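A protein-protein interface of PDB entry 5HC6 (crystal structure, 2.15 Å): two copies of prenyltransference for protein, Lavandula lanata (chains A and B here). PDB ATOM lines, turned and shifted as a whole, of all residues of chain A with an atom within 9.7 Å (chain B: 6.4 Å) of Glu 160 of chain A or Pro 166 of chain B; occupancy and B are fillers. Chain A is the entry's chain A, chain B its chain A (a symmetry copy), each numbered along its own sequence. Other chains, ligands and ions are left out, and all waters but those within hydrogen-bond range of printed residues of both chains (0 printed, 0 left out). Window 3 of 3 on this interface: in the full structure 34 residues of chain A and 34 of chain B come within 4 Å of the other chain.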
ATOM      1  N   VAL A 149      12.595 -22.315 -20.077  1.00  0.00           N
ATOM      2  CA  VAL A 149      12.755 -23.550 -19.342  1.00  0.00           C
ATOM      3  C   VAL A 149      13.346 -23.242 -17.963  1.00  0.00           C
ATOM      4  O   VAL A 149      12.872 -23.728 -16.928  1.00  0.00           O
ATOM      5  CB  VAL A 149      13.622 -24.607 -20.121  1.00  0.00           C
ATOM      6  CG1 VAL A 149      13.982 -25.805 -19.220  1.00  0.00           C
ATOM      7  CG2 VAL A 149      12.853 -25.119 -21.324  1.00  0.00           C
ATOM      8  N   GLU A 150      14.376 -22.426 -17.957  1.00  0.00           N
ATOM      9  CA  GLU A 150      14.996 -22.041 -16.682  1.00  0.00           C
ATOM     10  C   GLU A 150      14.008 -21.267 -15.802  1.00  0.00           C
ATOM     11  O   GLU A 150      13.949 -21.478 -14.607  1.00  0.00           O
ATOM     12  CB  GLU A 150      16.242 -21.250 -16.951  1.00  0.00           C
ATOM     13  CG  GLU A 150      16.893 -20.661 -15.711  1.00  0.00           C
ATOM     14  CD  GLU A 150      17.468 -21.723 -14.772  1.00  0.00           C
ATOM     15  OE1 GLU A 150      17.699 -22.855 -15.218  1.00  0.00           O
ATOM     16  OE2 GLU A 150      17.689 -21.396 -13.590  1.00  0.00           O
ATOM     17  N   ALA A 151      13.206 -20.377 -16.365  1.00  0.00           N
ATOM     18  CA  ALA A 151      12.200 -19.732 -15.529  1.00  0.00           C
ATOM     19  C   ALA A 151      11.295 -20.778 -14.888  1.00  0.00           C
ATOM     20  O   ALA A 151      10.975 -20.692 -13.712  1.00  0.00           O
ATOM     21  CB  ALA A 151      11.368 -18.716 -16.307  1.00  0.00           C
ATOM     22  N   ALA A 152      10.889 -21.771 -15.668  1.00  0.00           N
ATOM     23  CA  ALA A 152       9.937 -22.742 -15.172  1.00  0.00           C
ATOM     24  C   ALA A 152      10.585 -23.629 -14.083  1.00  0.00           C
ATOM     25  O   ALA A 152       9.919 -24.088 -13.189  1.00  0.00           O
ATOM     26  CB  ALA A 152       9.390 -23.576 -16.303  1.00  0.00           C
ATOM     27  N   ARG A 153      11.887 -23.836 -14.194  1.00  0.00           N
ATOM     28  CA  ARG A 153      12.637 -24.630 -13.265  1.00  0.00           C
ATOM     29  C   ARG A 153      12.693 -23.927 -11.934  1.00  0.00           C
ATOM     30  O   ARG A 153      12.475 -24.541 -10.878  1.00  0.00           O
ATOM     31  CB  ARG A 153      14.056 -24.775 -13.760  1.00  0.00           C
ATOM     32  CG  ARG A 153      14.300 -25.907 -14.698  1.00  0.00           C
ATOM     33  CD  ARG A 153      15.789 -26.222 -14.746  1.00  0.00           C
ATOM     34  NE  ARG A 153      15.947 -27.595 -15.185  1.00  0.00           N
ATOM     35  CZ  ARG A 153      16.492 -27.998 -16.329  1.00  0.00           C
ATOM     36  NH1 ARG A 153      17.007 -27.140 -17.202  1.00  0.00           N
ATOM     37  NH2 ARG A 153      16.536 -29.299 -16.591  1.00  0.00           N
ATOM     38  N   LYS A 154      13.000 -22.630 -11.997  1.00  0.00           N
ATOM     39  CA  LYS A 154      13.070 -21.815 -10.809  1.00  0.00           C
ATOM     40  C   LYS A 154      11.745 -21.757 -10.133  1.00  0.00           C
ATOM     41  O   LYS A 154      11.653 -21.920  -8.944  1.00  0.00           O
ATOM     42  CB  LYS A 154      13.528 -20.409 -11.136  1.00  0.00           C
ATOM     43  CG  LYS A 154      14.983 -20.382 -11.465  1.00  0.00           C
ATOM     44  CD  LYS A 154      15.332 -19.027 -12.062  1.00  0.00           C
ATOM     45  CE  LYS A 154      16.825 -18.921 -12.336  1.00  0.00           C
ATOM     46  NZ  LYS A 154      17.182 -17.516 -12.148  1.00  0.00           N
ATOM     47  N   ILE A 155      10.695 -21.517 -10.888  1.00  0.00           N
ATOM     48  CA  ILE A 155       9.363 -21.463 -10.281  1.00  0.00           C
ATOM     49  C   ILE A 155       9.007 -22.806  -9.615  1.00  0.00           C
ATOM     50  O   ILE A 155       8.319 -22.838  -8.612  1.00  0.00           O
ATOM     51  CB  ILE A 155       8.312 -21.096 -11.325  1.00  0.00           C
ATOM     52  CG1 ILE A 155       8.315 -19.578 -11.591  1.00  0.00           C
ATOM     53  CG2 ILE A 155       6.933 -21.512 -10.923  1.00  0.00           C
ATOM     54  CD1 ILE A 155       7.614 -19.199 -12.890  1.00  0.00           C
ATOM     55  N   ALA A 156       9.434 -23.898 -10.242  1.00  0.00           N
ATOM     56  CA  ALA A 156       9.120 -25.216  -9.821  1.00  0.00           C
ATOM     57  C   ALA A 156       9.805 -25.511  -8.463  1.00  0.00           C
ATOM     58  O   ALA A 156       9.156 -26.020  -7.562  1.00  0.00           O
ATOM     59  CB  ALA A 156       9.566 -26.199 -10.898  1.00  0.00           C
ATOM     60  N   ALA A 157      11.094 -25.177  -8.352  1.00  0.00           N
ATOM     61  CA  ALA A 157      11.853 -25.233  -7.107  1.00  0.00           C
ATOM     62  C   ALA A 157      11.177 -24.493  -5.959  1.00  0.00           C
ATOM     63  O   ALA A 157      11.182 -24.969  -4.812  1.00  0.00           O
ATOM     64  CB  ALA A 157      13.223 -24.637  -7.316  1.00  0.00           C
ATOM     65  N   LYS A 158      10.623 -23.321  -6.265  1.00  0.00           N
ATOM     66  CA  LYS A 158       9.922 -22.522  -5.259  1.00  0.00           C
ATOM     67  C   LYS A 158       8.619 -23.169  -4.907  1.00  0.00           C
ATOM     68  O   LYS A 158       8.153 -23.027  -3.787  1.00  0.00           O
ATOM     69  CB  LYS A 158       9.628 -21.106  -5.736  1.00  0.00           C
ATOM     70  CG  LYS A 158      10.830 -20.200  -5.848  1.00  0.00           C
ATOM     71  CD  LYS A 158      10.327 -18.748  -5.975  1.00  0.00           C
ATOM     72  CE  LYS A 158      11.466 -17.745  -6.174  1.00  0.00           C
ATOM     73  NZ  LYS A 158      10.946 -16.379  -6.442  1.00  0.00           N
ATOM     74  N   VAL A 159       8.011 -23.872  -5.861  1.00  0.00           N
ATOM     75  CA  VAL A 159       6.757 -24.561  -5.571  1.00  0.00           C
ATOM     76  C   VAL A 159       7.060 -25.702  -4.621  1.00  0.00           C
ATOM     77  O   VAL A 159       6.316 -25.912  -3.685  1.00  0.00           O
ATOM     78  CB  VAL A 159       5.996 -25.055  -6.827  1.00  0.00           C
ATOM     79  CG1 VAL A 159       4.896 -26.077  -6.481  1.00  0.00           C
ATOM     80  CG2 VAL A 159       5.349 -23.886  -7.540  1.00  0.00           C
ATOM     81  N   GLU A 160       8.163 -26.405  -4.868  1.00  0.00           N
ATOM     82  CA  GLU A 160       8.520 -27.560  -4.077  1.00  0.00           C
ATOM     83  C   GLU A 160       8.910 -27.148  -2.630  1.00  0.00           C
ATOM     84  O   GLU A 160       8.596 -27.860  -1.692  1.00  0.00           O
ATOM     85  CB  GLU A 160       9.604 -28.358  -4.797  1.00  0.00           C
ATOM     86  CG  GLU A 160      10.636 -29.052  -3.938  1.00  0.00           C
ATOM     87  CD  GLU A 160      11.667 -29.768  -4.790  1.00  0.00           C
ATOM     88  OE1 GLU A 160      12.776 -29.215  -4.969  1.00  0.00           O
ATOM     89  OE2 GLU A 160      11.347 -30.868  -5.307  1.00  0.00           O
ATOM     90  N   HIS A 161       9.537 -25.988  -2.456  1.00  0.00           N
ATOM     91  CA  HIS A 161       9.799 -25.455  -1.121  1.00  0.00           C
ATOM     92  C   HIS A 161       8.624 -24.634  -0.510  1.00  0.00           C
ATOM     93  O   HIS A 161       8.862 -23.835   0.366  1.00  0.00           O
ATOM     94  CB  HIS A 161      11.068 -24.576  -1.138  1.00  0.00           C
ATOM     95  CG  HIS A 161      12.313 -25.296  -1.560  1.00  0.00           C
ATOM     96  ND1 HIS A 161      13.309 -24.689  -2.297  1.00  0.00           N
ATOM     97  CD2 HIS A 161      12.734 -26.564  -1.338  1.00  0.00           C
ATOM     98  CE1 HIS A 161      14.284 -25.554  -2.515  1.00  0.00           C
ATOM     99  NE2 HIS A 161      13.963 -26.696  -1.937  1.00  0.00           N
ATOM    100  N   GLY A 162       7.382 -24.781  -0.968  1.00  0.00           N
ATOM    101  CA  GLY A 162       6.235 -24.088  -0.336  1.00  0.00           C
ATOM    102  C   GLY A 162       6.098 -22.579  -0.512  1.00  0.00           C
ATOM    103  O   GLY A 162       5.082 -21.981  -0.164  1.00  0.00           O
ATOM    104  N   ILE A 163       7.121 -21.968  -1.078  1.00  0.00           N
ATOM    105  CA  ILE A 163       7.174 -20.532  -1.355  1.00  0.00           C
ATOM    106  C   ILE A 163       6.110 -20.019  -2.344  1.00  0.00           C
ATOM    107  O   ILE A 163       5.738 -18.847  -2.302  1.00  0.00           O
ATOM    108  CB  ILE A 163       8.558 -20.223  -1.953  1.00  0.00           C
ATOM    109  CG1 ILE A 163       9.652 -20.570  -0.934  1.00  0.00           C
ATOM    110  CG2 ILE A 163       8.662 -18.773  -2.420  1.00  0.00           C
ATOM    111  CD1 ILE A 163      11.003 -20.833  -1.562  1.00  0.00           C
ATOM    112  N   LEU A 164       5.646 -20.892  -3.242  1.00  0.00           N
ATOM    113  CA  LEU A 164       4.680 -20.539  -4.278  1.00  0.00           C
ATOM    114  C   LEU A 164       3.724 -21.708  -4.470  1.00  0.00           C
ATOM    115  O   LEU A 164       4.152 -22.850  -4.405  1.00  0.00           O
ATOM    116  CB  LEU A 164       5.446 -20.311  -5.577  1.00  0.00           C
ATOM    117  CG  LEU A 164       5.346 -19.046  -6.407  1.00  0.00           C
ATOM    118  CD1 LEU A 164       5.172 -17.776  -5.602  1.00  0.00           C
ATOM    119  CD2 LEU A 164       6.611 -18.941  -7.245  1.00  0.00           C
ATOM    120  N   ARG A 165       2.456 -21.434  -4.748  1.00  0.00           N
ATOM    121  CA  ARG A 165       1.472 -22.476  -5.065  1.00  0.00           C
ATOM    122  C   ARG A 165       1.216 -22.449  -6.601  1.00  0.00           C
ATOM    123  O   ARG A 165       1.298 -21.389  -7.223  1.00  0.00           O
ATOM    124  CB  ARG A 165       0.179 -22.186  -4.313  1.00  0.00           C
ATOM    125  CG  ARG A 165      -0.593 -23.379  -3.733  1.00  0.00           C
ATOM    126  CD  ARG A 165      -1.384 -22.988  -2.474  1.00  0.00           C
ATOM    127  NE  ARG A 165      -2.437 -21.979  -2.719  1.00  0.00           N
ATOM    128  CZ  ARG A 165      -2.268 -20.648  -2.745  1.00  0.00           C
ATOM    129  NH1 ARG A 165      -1.075 -20.098  -2.546  1.00  0.00           N
ATOM    130  NH2 ARG A 165      -3.307 -19.852  -2.993  1.00  0.00           N
ATOM    131  N   PRO A 166       0.931 -23.611  -7.224  1.00  0.00           N
ATOM    132  CA  PRO A 166       0.681 -23.657  -8.664  1.00  0.00           C
ATOM    133  C   PRO A 166      -0.230 -22.544  -9.229  1.00  0.00           C
ATOM    134  O   PRO A 166       0.128 -21.914 -10.223  1.00  0.00           O
ATOM    135  CB  PRO A 166       0.076 -25.042  -8.843  1.00  0.00           C
ATOM    136  CG  PRO A 166       0.885 -25.840  -7.896  1.00  0.00           C
ATOM    137  CD  PRO A 166       0.966 -24.971  -6.664  1.00  0.00           C
ATOM    138  N   ILE A 169       0.876 -18.896 -10.243  1.00  0.00           N
ATOM    139  CA  ILE A 169       1.699 -18.669 -11.414  1.00  0.00           C
ATOM    140  C   ILE A 169       0.881 -17.885 -12.453  1.00  0.00           C
ATOM    141  O   ILE A 169      -0.159 -18.351 -12.918  1.00  0.00           O
ATOM    142  CB  ILE A 169       2.218 -20.003 -11.972  1.00  0.00           C
ATOM    143  CG1 ILE A 169       3.045 -20.696 -10.893  1.00  0.00           C
ATOM    144  CG2 ILE A 169       3.105 -19.772 -13.184  1.00  0.00           C
ATOM    145  CD1 ILE A 169       3.090 -22.192 -11.031  1.00  0.00           C
ATOM    146  N   VAL B 159       4.805 -31.002  -9.777  1.00  0.00           N
ATOM    147  CA  VAL B 159       5.972 -30.912  -8.905  1.00  0.00           C
ATOM    148  C   VAL B 159       5.493 -31.001  -7.471  1.00  0.00           C
ATOM    149  O   VAL B 159       6.107 -31.683  -6.677  1.00  0.00           O
ATOM    150  CB  VAL B 159       6.844 -29.651  -9.135  1.00  0.00           C
ATOM    151  CG1 VAL B 159       7.832 -29.405  -7.979  1.00  0.00           C
ATOM    152  CG2 VAL B 159       7.640 -29.792 -10.416  1.00  0.00           C
ATOM    153  N   GLU B 160       4.385 -30.326  -7.171  1.00  0.00           N
ATOM    154  CA  GLU B 160       3.869 -30.274  -5.823  1.00  0.00           C
ATOM    155  C   GLU B 160       3.338 -31.664  -5.374  1.00  0.00           C
ATOM    156  O   GLU B 160       3.496 -32.030  -4.223  1.00  0.00           O
ATOM    157  CB  GLU B 160       2.830 -29.161  -5.715  1.00  0.00           C
ATOM    158  CG  GLU B 160       1.665 -29.391  -4.781  1.00  0.00           C
ATOM    159  CD  GLU B 160       0.700 -28.221  -4.809  1.00  0.00           C
ATOM    160  OE1 GLU B 160      -0.346 -28.330  -5.489  1.00  0.00           O
ATOM    161  OE2 GLU B 160       1.011 -27.182  -4.175  1.00  0.00           O
ATOM    162  N   LEU B 164       7.023 -35.002 -10.418  1.00  0.00           N
ATOM    163  CA  LEU B 164       8.123 -34.425 -11.185  1.00  0.00           C
ATOM    164  C   LEU B 164       9.023 -33.647 -10.234  1.00  0.00           C
ATOM    165  O   LEU B 164       8.522 -33.010  -9.321  1.00  0.00           O
ATOM    166  CB  LEU B 164       7.529 -33.458 -12.203  1.00  0.00           C
ATOM    167  CG  LEU B 164       7.802 -33.526 -13.693  1.00  0.00           C
ATOM    168  CD1 LEU B 164       7.957 -34.928 -14.242  1.00  0.00           C
ATOM    169  CD2 LEU B 164       6.652 -32.831 -14.407  1.00  0.00           C
ATOM    170  N   ARG B 165      10.329 -33.658 -10.467  1.00  0.00           N
ATOM    171  CA  ARG B 165      11.278 -32.854  -9.688  1.00  0.00           C
ATOM    172  C   ARG B 165      11.714 -31.639 -10.560  1.00  0.00           C
ATOM    173  O   ARG B 165      11.769 -31.746 -11.786  1.00  0.00           O
ATOM    174  CB  ARG B 165      12.490 -33.711  -9.341  1.00  0.00           C
ATOM    175  CG  ARG B 165      13.115 -33.534  -7.951  1.00  0.00           C
ATOM    176  CD  ARG B 165      13.775 -34.832  -7.455  1.00  0.00           C
ATOM    177  NE  ARG B 165      14.908 -35.283  -8.290  1.00  0.00           N
ATOM    178  CZ  ARG B 165      14.824 -36.025  -9.405  1.00  0.00           C
ATOM    179  NH1 ARG B 165      13.652 -36.435  -9.876  1.00  0.00           N
ATOM    180  NH2 ARG B 165      15.931 -36.350 -10.071  1.00  0.00           N
ATOM    181  N   PRO B 166      11.998 -30.475  -9.941  1.00  0.00           N
ATOM    182  CA  PRO B 166      12.413 -29.295 -10.699  1.00  0.00           C
ATOM    183  C   PRO B 166      13.449 -29.539 -11.819  1.00  0.00           C
ATOM    184  O   PRO B 166      13.249 -29.078 -12.942  1.00  0.00           O
ATOM    185  CB  PRO B 166      12.949 -28.381  -9.607  1.00  0.00           C
ATOM    186  CG  PRO B 166      11.989 -28.637  -8.512  1.00  0.00           C
ATOM    187  CD  PRO B 166      11.816 -30.136  -8.521  1.00  0.00           C
ATOM    188  N   ASP B 167      14.492 -30.308 -11.548  1.00  0.00           N
ATOM    189  CA  ASP B 167      15.510 -30.566 -12.569  1.00  0.00           C
ATOM    190  C   ASP B 167      15.125 -31.582 -13.619  1.00  0.00           C
ATOM    191  O   ASP B 167      15.900 -31.819 -14.531  1.00  0.00           O
ATOM    192  CB  ASP B 167      16.812 -30.971 -11.935  1.00  0.00           C
ATOM    193  CG  ASP B 167      17.068 -30.192 -10.690  1.00  0.00           C
ATOM    194  OD1 ASP B 167      16.296 -30.433  -9.718  1.00  0.00           O
ATOM    195  OD2 ASP B 167      17.983 -29.324 -10.694  1.00  0.00           O
ATOM    196  N   ASP B 168      13.932 -32.152 -13.528  1.00  0.00           N
ATOM    197  CA  ASP B 168      13.407 -32.939 -14.628  1.00  0.00           C
ATOM    198  C   ASP B 168      12.766 -32.084 -15.704  1.00  0.00           C
ATOM    199  O   ASP B 168      12.326 -32.614 -16.722  1.00  0.00           O
ATOM    200  CB  ASP B 168      12.369 -33.966 -14.153  1.00  0.00           C
ATOM    201  CG  ASP B 168      12.916 -34.937 -13.067  1.00  0.00           C
ATOM    202  OD1 ASP B 168      14.179 -35.110 -12.881  1.00  0.00           O
ATOM    203  OD2 ASP B 168      12.022 -35.506 -12.396  1.00  0.00           O
ATOM    204  N   ILE B 169      12.691 -30.771 -15.489  1.00  0.00           N
ATOM    205  CA  ILE B 169      12.026 -29.904 -16.440  1.00  0.00           C
ATOM    206  C   ILE B 169      13.006 -29.566 -17.576  1.00  0.00           C
ATOM    207  O   ILE B 169      14.064 -28.980 -17.342  1.00  0.00           O
ATOM    208  CB  ILE B 169      11.497 -28.644 -15.738  1.00  0.00           C
ATOM    209  CG1 ILE B 169      10.509 -29.065 -14.655  1.00  0.00           C
ATOM    210  CG2 ILE B 169      10.774 -27.741 -16.724  1.00  0.00           C
ATOM    211  CD1 ILE B 169      10.391 -28.082 -13.526  1.00  0.00           C
ATOM    212  N   ASP B 170      12.661 -29.973 -18.790  1.00  0.00           N
ATOM    213  CA  ASP B 170      13.484 -29.655 -19.943  1.00  0.00           C
ATOM    214  C   ASP B 170      12.536 -29.248 -21.026  1.00  0.00           C
ATOM    215  O   ASP B 170      11.310 -29.294 -20.787  1.00  0.00           O
ATOM    216  CB  ASP B 170      14.372 -30.851 -20.332  1.00  0.00           C
ATOM    217  CG  ASP B 170      13.576 -32.123 -20.610  1.00  0.00           C
ATOM    218  OD1 ASP B 170      12.318 -32.110 -20.704  1.00  0.00           O
ATOM    219  OD2 ASP B 170      14.243 -33.160 -20.784  1.00  0.00           O
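Of the 9 printed residues of chain B, 6 touch a printed residue of chain A.
Hydrophobic or aromatic side chains of chain B that line the printed part of chain A: Val 159, Pro 166 and Ile 169.
Among the printed residues, no Asp or Glu carboxylate lies within 4 Å of a Lys or Arg side-chain nitrogen of the other chain.
NH2 of Arg 153 of chain A sits at hydrogen-bond distance from O of Ile 169 of chain B (2.6 Å).
NH2 of Arg 153 of chain A sits at hydrogen-bond distance from O of Asp 167 of chain B, 3.3 Å away.
Pro 166 of chain B touches four residues of chain A.
Of chain A, only Arg 153 comes within 4 Å of Asp 167 of chain B.
Ile 169 of chain B touches just these residues of chain A: Val 149 (3.7 Å), Arg 153 (2.6 Å) and Ala 156 (3.3 Å).
Printed residues of chain B within 4 Å of Val 159 of chain A: Glu 160 (3.8 Å).
Printed residues of chain A within 4 Å of Asp 170 of chain B: Val 149 (3.9 Å).
The nearest residue of chain A that does not touch Pro 166 of chain B is Lys 158 of chain A (5.9 Å).
The nearest printed residue of chain A that does not touch Asp 170 of chain B is Arg 153 of chain A (4.5 Å).
The backbone carbonyl oxygen (O) of Ala 157 of chain A is in hydrogen-bond range of a ring nitrogen (ND1) of His 161 of chain A (3.3 Å).
Val 159 of chain A touches Glu 160 of chain B, and with the chains exchanged Glu 160 of chain A touches Val 159 of chain B.
Glu 160 of chain A touches Pro 166 of chain B, and with the chains exchanged Pro 166 of chain A touches Glu 160 of chain B.
Of the 13 pairs that touch across the chains among the printed residues, 4 have their exchanged pair printed and touching as well.
Val 149 of chain A touches Ile 169 of chain B.
Val 149 of chain A touches Asp 170 of chain B (CG1 to CA, 3.9 Å).
CG of Arg 153 of chain A touches O of Pro 166 of chain B, 3.8 Å away.
Val 159 of chain B touches Ala 156 of chain A (CG1 to O, 3.7 Å).
Pro 166 of chain B touches Ala 156 of chain A.
CD1 of Ile 169 of chain B touches CB of Ala 156 of chain A, 3.3 Å away.
Val 159 of chain A touches Glu 160 of chain B (CG1 to CB, 3.8 Å).
Glu 160 of chain A touches Val 159 of chain B.
Glu 160 of chain A touches Pro 166 of chain B (OE2 to CD, 3.3 Å).
Pro 166 of chain A touches Glu 160 of chain B.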
